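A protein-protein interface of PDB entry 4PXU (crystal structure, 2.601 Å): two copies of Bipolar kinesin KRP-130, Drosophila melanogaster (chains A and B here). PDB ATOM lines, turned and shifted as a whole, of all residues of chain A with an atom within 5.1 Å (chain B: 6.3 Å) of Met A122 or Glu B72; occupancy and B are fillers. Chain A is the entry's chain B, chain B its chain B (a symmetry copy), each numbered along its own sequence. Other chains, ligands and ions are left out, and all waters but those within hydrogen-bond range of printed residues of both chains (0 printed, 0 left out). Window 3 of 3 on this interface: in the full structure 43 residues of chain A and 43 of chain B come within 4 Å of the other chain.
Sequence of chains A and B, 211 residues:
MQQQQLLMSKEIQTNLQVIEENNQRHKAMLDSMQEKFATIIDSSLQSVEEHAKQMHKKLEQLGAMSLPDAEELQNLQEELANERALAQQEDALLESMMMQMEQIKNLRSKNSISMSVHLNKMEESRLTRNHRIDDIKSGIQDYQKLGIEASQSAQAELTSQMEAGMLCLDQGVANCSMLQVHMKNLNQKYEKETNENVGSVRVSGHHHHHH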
ATOM      1  N   VAL A 117      14.499  12.494  19.566  1.00  0.00           N
ATOM      2  CA  VAL A 117      15.544  13.477  19.308  1.00  0.00           C
ATOM      3  C   VAL A 117      16.288  13.217  17.991  1.00  0.00           C
ATOM      4  O   VAL A 117      16.418  14.126  17.156  1.00  0.00           O
ATOM      5  CB  VAL A 117      16.555  13.497  20.455  1.00  0.00           C
ATOM      6  CG1 VAL A 117      17.844  14.182  20.023  1.00  0.00           C
ATOM      7  CG2 VAL A 117      15.956  14.194  21.663  1.00  0.00           C
ATOM      8  N   HIS A 118      16.742  11.981  17.780  1.00  0.00           N
ATOM      9  CA  HIS A 118      17.451  11.655  16.541  1.00  0.00           C
ATOM     10  C   HIS A 118      16.543  11.777  15.318  1.00  0.00           C
ATOM     11  O   HIS A 118      16.997  12.184  14.245  1.00  0.00           O
ATOM     12  CB  HIS A 118      18.051  10.249  16.585  1.00  0.00           C
ATOM     13  CG  HIS A 118      19.198  10.115  17.540  1.00  0.00           C
ATOM     14  ND1 HIS A 118      19.038   9.695  18.839  1.00  0.00           N
ATOM     15  CD2 HIS A 118      20.511  10.409  17.391  1.00  0.00           C
ATOM     16  CE1 HIS A 118      20.218   9.697  19.446  1.00  0.00           C
ATOM     17  NE2 HIS A 118      21.122  10.126  18.591  1.00  0.00           N
ATOM     18  N   LEU A 119      15.265  11.440  15.477  1.00  0.00           N
ATOM     19  CA  LEU A 119      14.307  11.605  14.387  1.00  0.00           C
ATOM     20  C   LEU A 119      14.130  13.083  14.044  1.00  0.00           C
ATOM     21  O   LEU A 119      13.953  13.440  12.878  1.00  0.00           O
ATOM     22  CB  LEU A 119      12.944  11.002  14.747  1.00  0.00           C
ATOM     23  CG  LEU A 119      12.832   9.488  14.870  1.00  0.00           C
ATOM     24  CD1 LEU A 119      11.382   9.121  15.129  1.00  0.00           C
ATOM     25  CD2 LEU A 119      13.361   8.798  13.617  1.00  0.00           C
ATOM     26  N   ASN A 120      14.194  13.948  15.051  1.00  0.00           N
ATOM     27  CA  ASN A 120      14.040  15.366  14.776  1.00  0.00           C
ATOM     28  C   ASN A 120      15.273  15.910  14.075  1.00  0.00           C
ATOM     29  O   ASN A 120      15.171  16.764  13.194  1.00  0.00           O
ATOM     30  CB  ASN A 120      13.784  16.141  16.061  1.00  0.00           C
ATOM     31  CG  ASN A 120      12.450  15.794  16.686  1.00  0.00           C
ATOM     32  OD1 ASN A 120      11.499  15.435  15.988  1.00  0.00           O
ATOM     33  ND2 ASN A 120      12.376  15.881  18.016  1.00  0.00           N
ATOM     34  N   LYS A 121      16.434  15.375  14.439  1.00  0.00           N
ATOM     35  CA  LYS A 121      17.664  15.793  13.804  1.00  0.00           C
ATOM     36  C   LYS A 121      17.613  15.390  12.343  1.00  0.00           C
ATOM     37  O   LYS A 121      17.945  16.186  11.464  1.00  0.00           O
ATOM     38  CB  LYS A 121      18.894  15.206  14.500  1.00  0.00           C
ATOM     39  CG  LYS A 121      20.122  16.076  14.295  1.00  0.00           C
ATOM     40  CD  LYS A 121      19.918  17.449  14.927  1.00  0.00           C
ATOM     41  CE  LYS A 121      21.104  18.378  14.706  1.00  0.00           C
ATOM     42  NZ  LYS A 121      20.901  19.152  13.443  1.00  0.00           N
ATOM     43  N   MET A 122      17.167  14.166  12.083  1.00  0.00           N
ATOM     44  CA  MET A 122      17.088  13.680  10.713  1.00  0.00           C
ATOM     45  C   MET A 122      16.100  14.493   9.886  1.00  0.00           C
ATOM     46  O   MET A 122      16.293  14.676   8.681  1.00  0.00           O
ATOM     47  CB  MET A 122      16.711  12.205  10.693  1.00  0.00           C
ATOM     48  CG  MET A 122      17.766  11.339  11.345  1.00  0.00           C
ATOM     49  SD  MET A 122      17.354   9.593  11.328  1.00  0.00           S
ATOM     50  CE  MET A 122      18.160   9.113   9.795  1.00  0.00           C
ATOM     51  N   GLU A 123      15.040  14.973  10.522  1.00  0.00           N
ATOM     52  CA  GLU A 123      14.087  15.823   9.820  1.00  0.00           C
ATOM     53  C   GLU A 123      14.693  17.180   9.443  1.00  0.00           C
ATOM     54  O   GLU A 123      14.377  17.733   8.393  1.00  0.00           O
ATOM     55  CB  GLU A 123      12.827  16.011  10.667  1.00  0.00           C
ATOM     56  CG  GLU A 123      11.780  16.959  10.079  1.00  0.00           C
ATOM     57  CD  GLU A 123      11.426  16.642   8.631  1.00  0.00           C
ATOM     58  OE1 GLU A 123      11.508  15.466   8.216  1.00  0.00           O
ATOM     59  OE2 GLU A 123      11.034  17.581   7.910  1.00  0.00           O
ATOM     60  N   GLU A 124      15.568  17.707  10.297  1.00  0.00           N
ATOM     61  CA  GLU A 124      16.287  18.944   9.989  1.00  0.00           C
ATOM     62  C   GLU A 124      17.276  18.731   8.851  1.00  0.00           C
ATOM     63  O   GLU A 124      17.357  19.529   7.916  1.00  0.00           O
ATOM     64  CB  GLU A 124      17.021  19.466  11.221  1.00  0.00           C
ATOM     65  CG  GLU A 124      16.145  20.281  12.160  1.00  0.00           C
ATOM     66  CD  GLU A 124      16.859  20.641  13.454  1.00  0.00           C
ATOM     67  OE1 GLU A 124      18.064  20.977  13.387  1.00  0.00           O
ATOM     68  OE2 GLU A 124      16.222  20.571  14.534  1.00  0.00           O
ATOM     69  N   SER A 125      18.037  17.648   8.945  1.00  0.00           N
ATOM     70  CA  SER A 125      18.997  17.298   7.917  1.00  0.00           C
ATOM     71  C   SER A 125      18.322  17.025   6.563  1.00  0.00           C
ATOM     72  O   SER A 125      18.950  17.142   5.509  1.00  0.00           O
ATOM     73  CB  SER A 125      19.810  16.087   8.358  1.00  0.00           C
ATOM     74  OG  SER A 125      20.681  15.648   7.326  1.00  0.00           O
ATOM     75  N   ARG A 126      17.041  16.679   6.581  1.00  0.00           N
ATOM     76  CA  ARG A 126      16.333  16.444   5.331  1.00  0.00           C
ATOM     77  C   ARG A 126      15.884  17.774   4.727  1.00  0.00           C
ATOM     78  O   ARG A 126      15.988  17.984   3.519  1.00  0.00           O
ATOM     79  CB  ARG A 126      15.132  15.532   5.542  1.00  0.00           C
ATOM     80  CG  ARG A 126      14.420  15.136   4.262  1.00  0.00           C
ATOM     81  CD  ARG A 126      13.102  14.411   4.552  1.00  0.00           C
ATOM     82  NE  ARG A 126      12.158  15.315   5.203  1.00  0.00           N
ATOM     83  CZ  ARG A 126      11.319  16.110   4.547  1.00  0.00           C
ATOM     84  NH1 ARG A 126      11.313  16.116   3.223  1.00  0.00           N
ATOM     85  NH2 ARG A 126      10.497  16.909   5.212  1.00  0.00           N
ATOM     86  N   LEU B  67      27.624  11.718   6.281  1.00  0.00           N
ATOM     87  CA  LEU B  67      28.215  11.178   7.506  1.00  0.00           C
ATOM     88  C   LEU B  67      27.353  11.415   8.756  1.00  0.00           C
ATOM     89  O   LEU B  67      27.107  10.472   9.503  1.00  0.00           O
ATOM     90  CB  LEU B  67      29.626  11.739   7.716  1.00  0.00           C
ATOM     91  CG  LEU B  67      30.580  10.824   8.489  1.00  0.00           C
ATOM     92  CD1 LEU B  67      30.831   9.541   7.711  1.00  0.00           C
ATOM     93  CD2 LEU B  67      31.890  11.549   8.793  1.00  0.00           C
ATOM     94  N   PRO B  68      26.883  12.660   8.995  1.00  0.00           N
ATOM     95  CA  PRO B  68      25.943  12.791  10.118  1.00  0.00           C
ATOM     96  C   PRO B  68      24.656  11.972   9.939  1.00  0.00           C
ATOM     97  O   PRO B  68      24.113  11.455  10.922  1.00  0.00           O
ATOM     98  CB  PRO B  68      25.630  14.292  10.131  1.00  0.00           C
ATOM     99  CG  PRO B  68      26.840  14.925   9.536  1.00  0.00           C
ATOM    100  CD  PRO B  68      27.250  13.979   8.445  1.00  0.00           C
ATOM    101  N   ASP B  69      24.194  11.845   8.697  1.00  0.00           N
ATOM    102  CA  ASP B  69      23.022  11.031   8.382  1.00  0.00           C
ATOM    103  C   ASP B  69      23.272   9.588   8.785  1.00  0.00           C
ATOM    104  O   ASP B  69      22.402   8.932   9.349  1.00  0.00           O
ATOM    105  CB  ASP B  69      22.681  11.110   6.888  1.00  0.00           C
ATOM    106  CG  ASP B  69      22.017  12.428   6.496  1.00  0.00           C
ATOM    107  OD1 ASP B  69      21.640  13.209   7.392  1.00  0.00           O
ATOM    108  OD2 ASP B  69      21.911  12.702   5.280  1.00  0.00           O
ATOM    109  N   ALA B  70      24.477   9.106   8.503  1.00  0.00           N
ATOM    110  CA  ALA B  70      24.852   7.732   8.818  1.00  0.00           C
ATOM    111  C   ALA B  70      24.952   7.551  10.321  1.00  0.00           C
ATOM    112  O   ALA B  70      24.620   6.489  10.860  1.00  0.00           O
ATOM    113  CB  ALA B  70      26.172   7.373   8.150  1.00  0.00           C
ATOM    114  N   GLU B  71      25.389   8.623  10.980  1.00  0.00           N
ATOM    115  CA  GLU B  71      25.545   8.676  12.429  1.00  0.00           C
ATOM    116  C   GLU B  71      24.203   8.521  13.130  1.00  0.00           C
ATOM    117  O   GLU B  71      24.062   7.767  14.096  1.00  0.00           O
ATOM    118  CB  GLU B  71      26.176  10.012  12.835  1.00  0.00           C
ATOM    119  CG  GLU B  71      26.518  10.121  14.306  1.00  0.00           C
ATOM    120  CD  GLU B  71      27.773   9.348  14.656  1.00  0.00           C
ATOM    121  OE1 GLU B  71      28.603   9.135  13.738  1.00  0.00           O
ATOM    122  OE2 GLU B  71      27.917   8.941  15.834  1.00  0.00           O
ATOM    123  N   GLU B  72      23.214   9.243  12.621  1.00  0.00           N
ATOM    124  CA  GLU B  72      21.885   9.232  13.204  1.00  0.00           C
ATOM    125  C   GLU B  72      21.256   7.857  13.076  1.00  0.00           C
ATOM    126  O   GLU B  72      20.591   7.385  13.998  1.00  0.00           O
ATOM    127  CB  GLU B  72      21.003  10.292  12.545  1.00  0.00           C
ATOM    128  CG  GLU B  72      21.453  11.721  12.828  1.00  0.00           C
ATOM    129  CD  GLU B  72      21.403  12.053  14.311  1.00  0.00           C
ATOM    130  OE1 GLU B  72      20.294  12.058  14.880  1.00  0.00           O
ATOM    131  OE2 GLU B  72      22.468  12.316  14.909  1.00  0.00           O
ATOM    132  N   LEU B  73      21.475   7.218  11.930  1.00  0.00           N
ATOM    133  CA  LEU B  73      20.976   5.868  11.699  1.00  0.00           C
ATOM    134  C   LEU B  73      21.614   4.881  12.667  1.00  0.00           C
ATOM    135  O   LEU B  73      20.947   3.986  13.195  1.00  0.00           O
ATOM    136  CB  LEU B  73      21.239   5.436  10.260  1.00  0.00           C
ATOM    137  CG  LEU B  73      20.264   6.024   9.242  1.00  0.00           C
ATOM    138  CD1 LEU B  73      20.623   5.594   7.820  1.00  0.00           C
ATOM    139  CD2 LEU B  73      18.849   5.608   9.598  1.00  0.00           C
ATOM    140  N   GLN B  74      22.913   5.034  12.891  1.00  0.00           N
ATOM    141  CA  GLN B  74      23.603   4.141  13.804  1.00  0.00           C
ATOM    142  C   GLN B  74      23.065   4.313  15.215  1.00  0.00           C
ATOM    143  O   GLN B  74      22.948   3.346  15.956  1.00  0.00           O
ATOM    144  CB  GLN B  74      25.109   4.384  13.775  1.00  0.00           C
ATOM    145  CG  GLN B  74      25.905   3.394  14.611  1.00  0.00           C
ATOM    146  CD  GLN B  74      27.391   3.724  14.647  1.00  0.00           C
ATOM    147  OE1 GLN B  74      27.786   4.896  14.626  1.00  0.00           O
ATOM    148  NE2 GLN B  74      28.225   2.685  14.686  1.00  0.00           N
ATOM    149  N   ASN B  75      22.709   5.541  15.577  1.00  0.00           N
ATOM    150  CA  ASN B  75      22.131   5.776  16.894  1.00  0.00           C
ATOM    151  C   ASN B  75      20.766   5.114  17.034  1.00  0.00           C
ATOM    152  O   ASN B  75      20.531   4.391  17.999  1.00  0.00           O
ATOM    153  CB  ASN B  75      22.030   7.280  17.168  1.00  0.00           C
ATOM    154  CG  ASN B  75      23.385   7.909  17.450  1.00  0.00           C
ATOM    155  OD1 ASN B  75      24.271   7.261  18.008  1.00  0.00           O
ATOM    156  ND2 ASN B  75      23.564   9.157  17.036  1.00  0.00           N
ATOM    157  N   LEU B  76      19.887   5.315  16.053  1.00  0.00           N
ATOM    158  CA  LEU B  76      18.596   4.630  16.052  1.00  0.00           C
ATOM    159  C   LEU B  76      18.802   3.118  16.094  1.00  0.00           C
ATOM    160  O   LEU B  76      18.044   2.382  16.733  1.00  0.00           O
ATOM    161  CB  LEU B  76      17.770   5.012  14.826  1.00  0.00           C
ATOM    162  CG  LEU B  76      17.364   6.484  14.736  1.00  0.00           C
ATOM    163  CD1 LEU B  76      16.607   6.755  13.449  1.00  0.00           C
ATOM    164  CD2 LEU B  76      16.528   6.883  15.941  1.00  0.00           C
ATOM    165  N   GLN B  77      19.855   2.661  15.430  1.00  0.00           N
ATOM    166  CA  GLN B  77      20.160   1.244  15.397  1.00  0.00           C
ATOM    167  C   GLN B  77      20.530   0.749  16.796  1.00  0.00           C
ATOM    168  O   GLN B  77      20.110  -0.337  17.206  1.00  0.00           O
ATOM    169  CB  GLN B  77      21.287   0.974  14.397  1.00  0.00           C
ATOM    170  CG  GLN B  77      21.260  -0.423  13.806  1.00  0.00           C
ATOM    171  CD  GLN B  77      19.964  -0.712  13.082  1.00  0.00           C
ATOM    172  OE1 GLN B  77      19.649  -0.074  12.076  1.00  0.00           O
ATOM    173  NE2 GLN B  77      19.194  -1.674  13.600  1.00  0.00           N
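The side-chain amino group (NZ) of Lys A121 lies within salt-bridge range of the side-chain carboxylate (OE1) of Glu A124, 3.4 Å away.
The backbone carbonyl oxygen of Glu B71 lies within hydrogen-bond range of the side-chain amide nitrogen of Asn B75, 3.3 Å away.
No position is printed for both chains.
Of the 9 pairs that touch across the chains among the printed residues, none has its exchanged pair printed and touching as well.
Leu B76 touches His A118 (CD2 to CB, 3.8 Å).
Leu A119 touches Leu B76 (CD2 to CD1, 3.8 Å).
Lys A121 touches Glu B72.
Met A122 touches Glu B72 (CG to CB, 3.6 Å).
CE of Met A122 touches CD2 of Leu B73, 3.6 Å away.
Met A122 touches Leu B76 (SD to CD1, 3.6 Å).
OE1 of Glu B72 lies close to O of His A118, at 3.4 Å.
ND2 of Asn B75 is in hydrogen-bond range of NE2 of His A118.
OG of Ser A125 lies within hydrogen-bond range of OD1 of Asp B69 (2.6 Å).
Printed residues of chain B within 4 Å of His A118: Glu B72, Asn B75 and Leu B76.
Printed residues of chain B within 4 Å of Lys A121: Glu B72 (3.5 Å).
Of chain B, only Glu B72 (3.6 Å), Leu B73 (3.6 Å) and Leu B76 (3.6 Å) come within 4 Å of Met A122.
Glu A124 touches none of the printed residues of chain B.
Of the printed residues of chain A, Asp B69 touches Ser A125 (2.6 Å).
Glu B72 touches just these residues of chain A: His A118, Lys A121 and Met A122.
Of the printed residues of chain A, Leu B73 touches Met A122.
Printed residues of chain A within 4 Å of Asn B75: His A118 (3.1 Å).
Hydrophobic or aromatic side chains of chain B that line the printed part of chain A: Leu B73 and Leu B76.
Along chain B the printed residues that touch a printed residue of chain A span positions 69 to 76.
Of the 10 printed residues of chain A, 5 touch a printed residue of chain B.
Printed residues of chain A that touch a printed residue of chain B: His A118, Leu A119, Lys A121, Met A122 and Ser A125.
Among the printed residues, 9 pairs touch across the chains.
Among the printed residues, no Asp or Glu carboxylate lies within 4 Å of a Lys or Arg side-chain nitrogen of the other chain.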
